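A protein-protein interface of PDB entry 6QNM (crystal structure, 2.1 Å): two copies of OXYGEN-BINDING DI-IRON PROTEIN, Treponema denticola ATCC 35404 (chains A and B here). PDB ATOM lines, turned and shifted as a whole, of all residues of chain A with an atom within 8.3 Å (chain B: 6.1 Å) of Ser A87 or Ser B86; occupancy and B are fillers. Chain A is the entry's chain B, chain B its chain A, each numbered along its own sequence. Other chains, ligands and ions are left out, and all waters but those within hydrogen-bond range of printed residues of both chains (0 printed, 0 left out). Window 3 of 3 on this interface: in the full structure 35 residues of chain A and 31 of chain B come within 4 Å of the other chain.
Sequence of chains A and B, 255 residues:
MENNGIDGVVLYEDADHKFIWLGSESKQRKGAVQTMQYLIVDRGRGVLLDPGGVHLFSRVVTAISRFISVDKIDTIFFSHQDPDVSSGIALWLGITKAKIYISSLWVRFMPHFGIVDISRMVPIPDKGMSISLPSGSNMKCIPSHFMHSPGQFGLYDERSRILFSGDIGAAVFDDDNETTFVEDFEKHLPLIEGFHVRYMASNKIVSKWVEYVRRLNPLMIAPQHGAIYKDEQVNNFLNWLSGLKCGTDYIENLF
Asp A82 touches Pro B83, and with the chains exchanged Pro A83 touches Asp B82. Pro A83 touches Val B85, but with the chains exchanged Val A85 does not touch Pro B83 (6.1 Å). Pro A83 touches Ser B86, and with the chains exchanged Ser A86 touches Pro B83. Ser A87 touches Ser B86, but with the chains exchanged Ser A86 does not touch Ser B87 (7.0 Å). 11 positions are printed for both chains. Of the 7 pairs that touch across the chains among the printed residues, 5 have their exchanged pair printed and touching as well.
The backbone carbonyl oxygen of Pro A83 lies within hydrogen-bond range of the side-chain hydroxyl of Ser B86 (3.0 Å).
Among the printed residues, pairs that only touch across the chains: Pro A83 with Asp B82 (3.0 Å), Pro A83 with Pro B83 (3.2 Å), Ser A87 with Ser B86 (3.5 Å), Asp A82 with Pro B83 (3.8 Å), Ser A86 with Pro B83 (3.8 Å) and Pro A83 with Val B85 (3.9 Å).
Of the 19 printed residues of chain A, 4 touch a printed residue of chain B. Among the printed residues, 7 pairs touch across the chains. Among the printed residues, no Asp or Glu carboxylate lies within 4 Å of a Lys or Arg side-chain nitrogen of the other chain.
Printed residues of chain B within 4 Å of Pro A83: Asp B82 (3.0 Å), Pro B83 (3.2 Å), Val B85 (3.9 Å) and Ser B86 (3.0 Å). Printed residues of chain B within 4 Å of Ser A86: Pro B83. Ser A87 touches one residue of chain B. Val B85 touches one residue of chain A. Ser B86 touches two residues of chain A. The nearest printed residue of chain B that does not touch Asp A82 is Asp B82 (5.4 Å).
OD1 of Asp A82 lies close to N of Asp A84. The backbone NH of Asp B84 sits close to the side-chain carboxylate of Asp B82 (3.1 Å).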
ATOM      1  N   GLY A  52     -23.989 -26.968   8.090  1.00  0.00           N
ATOM      2  CA  GLY A  52     -22.606 -27.166   8.482  1.00  0.00           C
ATOM      3  C   GLY A  52     -21.756 -28.186   7.749  1.00  0.00           C
ATOM      4  O   GLY A  52     -21.117 -27.874   6.737  1.00  0.00           O
ATOM      5  N   GLY A  53     -21.762 -29.412   8.268  1.00  0.00           N
ATOM      6  CA  GLY A  53     -20.602 -30.283   8.150  1.00  0.00           C
ATOM      7  C   GLY A  53     -20.160 -30.553   6.723  1.00  0.00           C
ATOM      8  O   GLY A  53     -20.974 -30.790   5.825  1.00  0.00           O
ATOM      9  N   VAL A  54     -18.840 -30.502   6.522  1.00  0.00           N
ATOM     10  CA  VAL A  54     -18.242 -31.167   5.373  1.00  0.00           C
ATOM     11  C   VAL A  54     -18.228 -32.668   5.623  1.00  0.00           C
ATOM     12  O   VAL A  54     -18.647 -33.469   4.777  1.00  0.00           O
ATOM     13  CB  VAL A  54     -16.820 -30.627   5.118  1.00  0.00           C
ATOM     14  CG1 VAL A  54     -16.002 -31.627   4.305  1.00  0.00           C
ATOM     15  CG2 VAL A  54     -16.864 -29.271   4.430  1.00  0.00           C
ATOM     16  N   HIS A  55     -17.741 -33.067   6.803  1.00  0.00           N
ATOM     17  CA  HIS A  55     -17.756 -34.447   7.272  1.00  0.00           C
ATOM     18  C   HIS A  55     -19.157 -34.961   7.579  1.00  0.00           C
ATOM     19  O   HIS A  55     -19.320 -36.167   7.793  1.00  0.00           O
ATOM     20  CB  HIS A  55     -16.879 -34.565   8.519  1.00  0.00           C
ATOM     21  CG  HIS A  55     -16.474 -35.967   8.851  1.00  0.00           C
ATOM     22  ND1 HIS A  55     -17.070 -36.696   9.858  1.00  0.00           N
ATOM     23  CD2 HIS A  55     -15.528 -36.773   8.311  1.00  0.00           C
ATOM     24  CE1 HIS A  55     -16.510 -37.892   9.922  1.00  0.00           C
ATOM     25  NE2 HIS A  55     -15.572 -37.964   8.995  1.00  0.00           N
ATOM     26  N   PHE A  57     -21.980 -33.860   5.583  1.00  0.00           N
ATOM     27  CA  PHE A  57     -22.859 -33.522   4.467  1.00  0.00           C
ATOM     28  C   PHE A  57     -23.642 -34.744   3.991  1.00  0.00           C
ATOM     29  O   PHE A  57     -24.867 -34.693   3.847  1.00  0.00           O
ATOM     30  CB  PHE A  57     -22.039 -32.923   3.327  1.00  0.00           C
ATOM     31  CG  PHE A  57     -22.849 -32.612   2.100  1.00  0.00           C
ATOM     32  CD1 PHE A  57     -23.638 -31.472   2.037  1.00  0.00           C
ATOM     33  CD2 PHE A  57     -22.824 -33.464   1.009  1.00  0.00           C
ATOM     34  CE1 PHE A  57     -24.388 -31.193   0.907  1.00  0.00           C
ATOM     35  CE2 PHE A  57     -23.571 -33.190  -0.120  1.00  0.00           C
ATOM     36  CZ  PHE A  57     -24.352 -32.055  -0.173  1.00  0.00           C
ATOM     37  N   PHE A  78     -27.456 -19.807   8.461  1.00  0.00           N
ATOM     38  CA  PHE A  78     -26.222 -20.027   9.212  1.00  0.00           C
ATOM     39  C   PHE A  78     -26.139 -19.015  10.346  1.00  0.00           C
ATOM     40  O   PHE A  78     -26.179 -17.802  10.103  1.00  0.00           O
ATOM     41  CB  PHE A  78     -24.996 -19.910   8.307  1.00  0.00           C
ATOM     42  CG  PHE A  78     -24.773 -21.105   7.431  1.00  0.00           C
ATOM     43  CD1 PHE A  78     -24.461 -22.337   7.981  1.00  0.00           C
ATOM     44  CD2 PHE A  78     -24.872 -20.994   6.054  1.00  0.00           C
ATOM     45  CE1 PHE A  78     -24.251 -23.439   7.173  1.00  0.00           C
ATOM     46  CE2 PHE A  78     -24.664 -22.092   5.240  1.00  0.00           C
ATOM     47  CZ  PHE A  78     -24.353 -23.314   5.799  1.00  0.00           C
ATOM     48  N   ASP A  82     -17.906 -20.290  10.474  1.00  0.00           N
ATOM     49  CA  ASP A  82     -17.339 -21.539  10.961  1.00  0.00           C
ATOM     50  C   ASP A  82     -16.419 -22.111   9.890  1.00  0.00           C
ATOM     51  O   ASP A  82     -16.786 -22.068   8.706  1.00  0.00           O
ATOM     52  CB  ASP A  82     -18.466 -22.529  11.297  1.00  0.00           C
ATOM     53  CG  ASP A  82     -17.978 -23.789  11.992  1.00  0.00           C
ATOM     54  OD1 ASP A  82     -16.775 -23.920  12.284  1.00  0.00           O
ATOM     55  OD2 ASP A  82     -18.824 -24.664  12.259  1.00  0.00           O
ATOM     56  N   PRO A  83     -15.229 -22.619  10.237  1.00  0.00           N
ATOM     57  CA  PRO A  83     -14.428 -23.319   9.214  1.00  0.00           C
ATOM     58  C   PRO A  83     -15.182 -24.468   8.583  1.00  0.00           C
ATOM     59  O   PRO A  83     -14.806 -24.935   7.499  1.00  0.00           O
ATOM     60  CB  PRO A  83     -13.209 -23.830   9.992  1.00  0.00           C
ATOM     61  CG  PRO A  83     -13.159 -23.054  11.250  1.00  0.00           C
ATOM     62  CD  PRO A  83     -14.456 -22.333  11.463  1.00  0.00           C
ATOM     63  N   ASP A  84     -16.258 -24.913   9.227  1.00  0.00           N
ATOM     64  CA  ASP A  84     -17.168 -25.895   8.665  1.00  0.00           C
ATOM     65  C   ASP A  84     -18.324 -25.259   7.901  1.00  0.00           C
ATOM     66  O   ASP A  84     -18.879 -25.888   6.993  1.00  0.00           O
ATOM     67  CB  ASP A  84     -17.708 -26.759   9.799  1.00  0.00           C
ATOM     68  CG  ASP A  84     -18.419 -27.987   9.313  1.00  0.00           C
ATOM     69  OD1 ASP A  84     -17.946 -28.623   8.354  1.00  0.00           O
ATOM     70  OD2 ASP A  84     -19.468 -28.299   9.922  1.00  0.00           O
ATOM     71  N   VAL A  85     -18.654 -24.002   8.204  1.00  0.00           N
ATOM     72  CA  VAL A  85     -19.648 -23.267   7.440  1.00  0.00           C
ATOM     73  C   VAL A  85     -19.153 -23.018   6.037  1.00  0.00           C
ATOM     74  O   VAL A  85     -19.795 -23.421   5.067  1.00  0.00           O
ATOM     75  N   SER A  86     -18.007 -22.357   5.915  1.00  0.00           N
ATOM     76  CA  SER A  86     -17.315 -22.321   4.639  1.00  0.00           C
ATOM     77  C   SER A  86     -16.778 -23.714   4.309  1.00  0.00           C
ATOM     78  O   SER A  86     -16.566 -24.546   5.196  1.00  0.00           O
ATOM     79  CB  SER A  86     -16.189 -21.287   4.668  1.00  0.00           C
ATOM     80  OG  SER A  86     -16.563 -20.154   5.437  1.00  0.00           O
ATOM     81  N   SER A  87     -16.577 -23.958   3.005  1.00  0.00           N
ATOM     82  CA  SER A  87     -16.198 -25.247   2.414  1.00  0.00           C
ATOM     83  C   SER A  87     -17.438 -26.130   2.292  1.00  0.00           C
ATOM     84  O   SER A  87     -17.501 -27.027   1.441  1.00  0.00           O
ATOM     85  CB  SER A  87     -15.097 -25.960   3.216  1.00  0.00           C
ATOM     86  OG  SER A  87     -14.045 -25.076   3.558  1.00  0.00           O
ATOM     87  N   GLY A  88     -18.426 -25.861   3.144  1.00  0.00           N
ATOM     88  CA  GLY A  88     -19.705 -26.536   3.178  1.00  0.00           C
ATOM     89  C   GLY A  88     -20.704 -25.864   2.258  1.00  0.00           C
ATOM     90  O   GLY A  88     -21.506 -26.524   1.592  1.00  0.00           O
ATOM     91  N   ILE A  89     -20.663 -24.530   2.244  1.00  0.00           N
ATOM     92  CA  ILE A  89     -21.586 -23.737   1.434  1.00  0.00           C
ATOM     93  C   ILE A  89     -21.527 -24.156  -0.032  1.00  0.00           C
ATOM     94  O   ILE A  89     -22.562 -24.252  -0.703  1.00  0.00           O
ATOM     95  CB  ILE A  89     -21.276 -22.239   1.623  1.00  0.00           C
ATOM     96  CG1 ILE A  89     -21.811 -21.763   2.970  1.00  0.00           C
ATOM     97  CG2 ILE A  89     -21.857 -21.408   0.494  1.00  0.00           C
ATOM     98  CD1 ILE A  89     -21.679 -20.278   3.198  1.00  0.00           C
ATOM     99  N   ALA A  90     -20.325 -24.399  -0.558  1.00  0.00           N
ATOM    100  CA  ALA A  90     -20.195 -24.866  -1.936  1.00  0.00           C
ATOM    101  C   ALA A  90     -21.052 -26.104  -2.182  1.00  0.00           C
ATOM    102  O   ALA A  90     -21.742 -26.203  -3.205  1.00  0.00           O
ATOM    103  CB  ALA A  90     -18.730 -25.148  -2.268  1.00  0.00           C
ATOM    104  N   LEU A  91     -21.026 -27.055  -1.247  1.00  0.00           N
ATOM    105  CA  LEU A  91     -21.780 -28.296  -1.414  1.00  0.00           C
ATOM    106  C   LEU A  91     -23.282 -28.044  -1.407  1.00  0.00           C
ATOM    107  O   LEU A  91     -24.025 -28.665  -2.179  1.00  0.00           O
ATOM    108  CB  LEU A  91     -21.402 -29.287  -0.313  1.00  0.00           C
ATOM    109  CG  LEU A  91     -19.942 -29.738  -0.264  1.00  0.00           C
ATOM    110  CD1 LEU A  91     -19.746 -30.806   0.799  1.00  0.00           C
ATOM    111  CD2 LEU A  91     -19.496 -30.245  -1.624  1.00  0.00           C
ATOM    112  N   TRP A  92     -23.756 -27.163  -0.524  1.00  0.00           N
ATOM    113  CA  TRP A  92     -25.192 -26.900  -0.448  1.00  0.00           C
ATOM    114  C   TRP A  92     -25.689 -26.116  -1.655  1.00  0.00           C
ATOM    115  O   TRP A  92     -26.811 -26.346  -2.118  1.00  0.00           O
ATOM    116  CB  TRP A  92     -25.518 -26.172   0.854  1.00  0.00           C
ATOM    117  CG  TRP A  92     -25.428 -27.083   2.035  1.00  0.00           C
ATOM    118  CD1 TRP A  92     -24.511 -27.032   3.042  1.00  0.00           C
ATOM    119  CD2 TRP A  92     -26.271 -28.208   2.314  1.00  0.00           C
ATOM    120  NE1 TRP A  92     -24.739 -28.049   3.939  1.00  0.00           N
ATOM    121  CE2 TRP A  92     -25.813 -28.785   3.514  1.00  0.00           C
ATOM    122  CE3 TRP A  92     -27.372 -28.777   1.670  1.00  0.00           C
ATOM    123  CZ2 TRP A  92     -26.416 -29.904   4.081  1.00  0.00           C
ATOM    124  CZ3 TRP A  92     -27.971 -29.888   2.235  1.00  0.00           C
ATOM    125  CH2 TRP A  92     -27.491 -30.439   3.428  1.00  0.00           C
ATOM    126  N   MET A 110     -16.503 -13.686   1.472  1.00  0.00           N
ATOM    127  CA  MET A 110     -16.795 -14.909   0.737  1.00  0.00           C
ATOM    128  C   MET A 110     -16.147 -15.008  -0.642  1.00  0.00           C
ATOM    129  O   MET A 110     -16.042 -16.119  -1.176  1.00  0.00           O
ATOM    130  CB  MET A 110     -18.301 -15.084   0.669  1.00  0.00           C
ATOM    131  CG  MET A 110     -18.829 -15.593   1.992  1.00  0.00           C
ATOM    132  SD  MET A 110     -20.049 -16.852   1.693  1.00  0.00           S
ATOM    133  CE  MET A 110     -21.072 -15.866   0.646  1.00  0.00           C
ATOM    134  N   HIS A 112     -13.601 -15.976  -1.475  1.00  0.00           N
ATOM    135  CA  HIS A 112     -12.494 -16.758  -0.940  1.00  0.00           C
ATOM    136  C   HIS A 112     -12.651 -18.221  -1.340  1.00  0.00           C
ATOM    137  O   HIS A 112     -13.299 -18.536  -2.339  1.00  0.00           O
ATOM    138  CB  HIS A 112     -12.442 -16.648   0.589  1.00  0.00           C
ATOM    139  CG  HIS A 112     -11.606 -15.514   1.093  1.00  0.00           C
ATOM    140  ND1 HIS A 112     -11.478 -14.321   0.416  1.00  0.00           N
ATOM    141  CD2 HIS A 112     -10.859 -15.391   2.217  1.00  0.00           C
ATOM    142  CE1 HIS A 112     -10.685 -13.513   1.098  1.00  0.00           C
ATOM    143  NE2 HIS A 112     -10.296 -14.138   2.195  1.00  0.00           N
ATOM    144  N   ASP B  82     -10.386 -19.970  12.668  1.00  0.00           N
ATOM    145  CA  ASP B  82     -10.581 -19.169  11.475  1.00  0.00           C
ATOM    146  C   ASP B  82     -11.450 -19.958  10.508  1.00  0.00           C
ATOM    147  O   ASP B  82     -11.119 -21.109  10.169  1.00  0.00           O
ATOM    148  CB  ASP B  82      -9.208 -18.832  10.851  1.00  0.00           C
ATOM    149  CG  ASP B  82      -9.304 -17.924   9.628  1.00  0.00           C
ATOM    150  OD1 ASP B  82     -10.420 -17.619   9.158  1.00  0.00           O
ATOM    151  OD2 ASP B  82      -8.240 -17.509   9.124  1.00  0.00           O
ATOM    152  N   PRO B  83     -12.534 -19.355  10.007  1.00  0.00           N
ATOM    153  CA  PRO B  83     -13.394 -20.044   9.032  1.00  0.00           C
ATOM    154  C   PRO B  83     -12.670 -20.517   7.788  1.00  0.00           C
ATOM    155  O   PRO B  83     -13.253 -21.308   7.033  1.00  0.00           O
ATOM    156  CB  PRO B  83     -14.463 -18.990   8.702  1.00  0.00           C
ATOM    157  CG  PRO B  83     -13.910 -17.681   9.248  1.00  0.00           C
ATOM    158  CD  PRO B  83     -13.135 -18.089  10.454  1.00  0.00           C
ATOM    159  N   ASP B  84     -11.451 -20.031   7.548  1.00  0.00           N
ATOM    160  CA  ASP B  84     -10.519 -20.497   6.528  1.00  0.00           C
ATOM    161  C   ASP B  84     -10.708 -21.954   6.123  1.00  0.00           C
ATOM    162  O   ASP B  84     -11.539 -22.266   5.264  1.00  0.00           O
ATOM    163  CB  ASP B  84      -9.093 -20.281   7.042  1.00  0.00           C
ATOM    164  CG  ASP B  84      -8.038 -20.692   6.048  1.00  0.00           C
ATOM    165  OD1 ASP B  84      -7.229 -21.575   6.399  1.00  0.00           O
ATOM    166  OD2 ASP B  84      -8.018 -20.145   4.926  1.00  0.00           O
ATOM    167  N   VAL B  85      -9.905 -22.846   6.706  1.00  0.00           N
ATOM    168  CA  VAL B  85     -10.062 -24.267   6.497  1.00  0.00           C
ATOM    169  C   VAL B  85      -9.990 -24.991   7.830  1.00  0.00           C
ATOM    170  O   VAL B  85      -9.512 -24.430   8.817  1.00  0.00           O
ATOM    171  N   SER B  86     -10.451 -26.252   7.869  1.00  0.00           N
ATOM    172  CA  SER B  86     -10.851 -27.142   6.763  1.00  0.00           C
ATOM    173  C   SER B  86      -9.743 -27.259   5.731  1.00  0.00           C
ATOM    174  O   SER B  86      -8.599 -27.561   6.069  1.00  0.00           O
ATOM    175  CB  SER B  86     -12.156 -26.688   6.092  1.00  0.00           C
ATOM    176  OG  SER B  86     -13.277 -27.342   6.665  1.00  0.00           O
ATOM    177  N   SER B  87     -10.089 -27.029   4.471  1.00  0.00           N
ATOM    178  CA  SER B  87      -9.076 -27.135   3.431  1.00  0.00           C
ATOM    179  C   SER B  87      -8.072 -26.010   3.646  1.00  0.00           C
ATOM    180  O   SER B  87      -8.305 -24.862   3.253  1.00  0.00           O
ATOM    181  CB  SER B  87      -9.692 -27.063   2.035  1.00  0.00           C
ATOM    182  OG  SER B  87     -10.450 -28.229   1.758  1.00  0.00           O
ATOM    183  N   GLY B  88      -6.984 -26.333   4.341  1.00  0.00           N
ATOM    184  CA  GLY B  88      -5.889 -25.416   4.589  1.00  0.00           C
ATOM    185  C   GLY B  88      -4.942 -25.975   5.626  1.00  0.00           C
ATOM    186  O   GLY B  88      -3.744 -26.101   5.367  1.00  0.00           O
ATOM    187  N   ILE B  89      -5.478 -26.375   6.781  1.00  0.00           N
ATOM    188  CA  ILE B  89      -4.646 -27.017   7.794  1.00  0.00           C
ATOM    189  C   ILE B  89      -4.138 -28.355   7.284  1.00  0.00           C
ATOM    190  O   ILE B  89      -2.973 -28.717   7.493  1.00  0.00           O
ATOM    191  CB  ILE B  89      -5.411 -27.185   9.119  1.00  0.00           C
ATOM    192  CG1 ILE B  89      -6.277 -25.956   9.409  1.00  0.00           C
ATOM    193  CG2 ILE B  89      -4.429 -27.462  10.243  1.00  0.00           C
ATOM    194  CD1 ILE B  89      -7.478 -26.266  10.274  1.00  0.00           C
ATOM    195  N   ALA B  90      -5.018 -29.115   6.621  1.00  0.00           N
ATOM    196  CA  ALA B  90      -4.688 -30.456   6.143  1.00  0.00           C
ATOM    197  C   ALA B  90      -3.393 -30.471   5.339  1.00  0.00           C
ATOM    198  O   ALA B  90      -2.532 -31.336   5.546  1.00  0.00           O
ATOM    199  CB  ALA B  90      -5.845 -31.001   5.305  1.00  0.00           C
ATOM    200  N   LEU B  91      -3.240 -29.521   4.413  1.00  0.00           N
ATOM    201  CA  LEU B  91      -2.036 -29.491   3.597  1.00  0.00           C
ATOM    202  C   LEU B  91      -0.816 -29.147   4.440  1.00  0.00           C
ATOM    203  O   LEU B  91       0.238 -29.771   4.302  1.00  0.00           O
ATOM    204  CB  LEU B  91      -2.192 -28.484   2.458  1.00  0.00           C
ATOM    205  CG  LEU B  91      -3.454 -28.549   1.596  1.00  0.00           C
ATOM    206  CD1 LEU B  91      -4.592 -27.745   2.200  1.00  0.00           C
ATOM    207  CD2 LEU B  91      -3.150 -28.058   0.201  1.00  0.00           C
ATOM    208  N   HIS B 112     -13.310 -30.714  13.235  1.00  0.00           N
ATOM    209  CA  HIS B 112     -14.623 -30.534  12.621  1.00  0.00           C
ATOM    210  C   HIS B 112     -14.493 -29.836  11.274  1.00  0.00           C
ATOM    211  O   HIS B 112     -13.624 -28.984  11.091  1.00  0.00           O
ATOM    212  CB  HIS B 112     -15.557 -29.753  13.549  1.00  0.00           C
ATOM    213  CG  HIS B 112     -16.248 -30.609  14.565  1.00  0.00           C
ATOM    214  ND1 HIS B 112     -16.135 -31.983  14.581  1.00  0.00           N
ATOM    215  CD2 HIS B 112     -17.057 -30.288  15.603  1.00  0.00           C
ATOM    216  CE1 HIS B 112     -16.845 -32.470  15.582  1.00  0.00           C
ATOM    217  NE2 HIS B 112     -17.415 -31.463  16.218  1.00  0.00           N
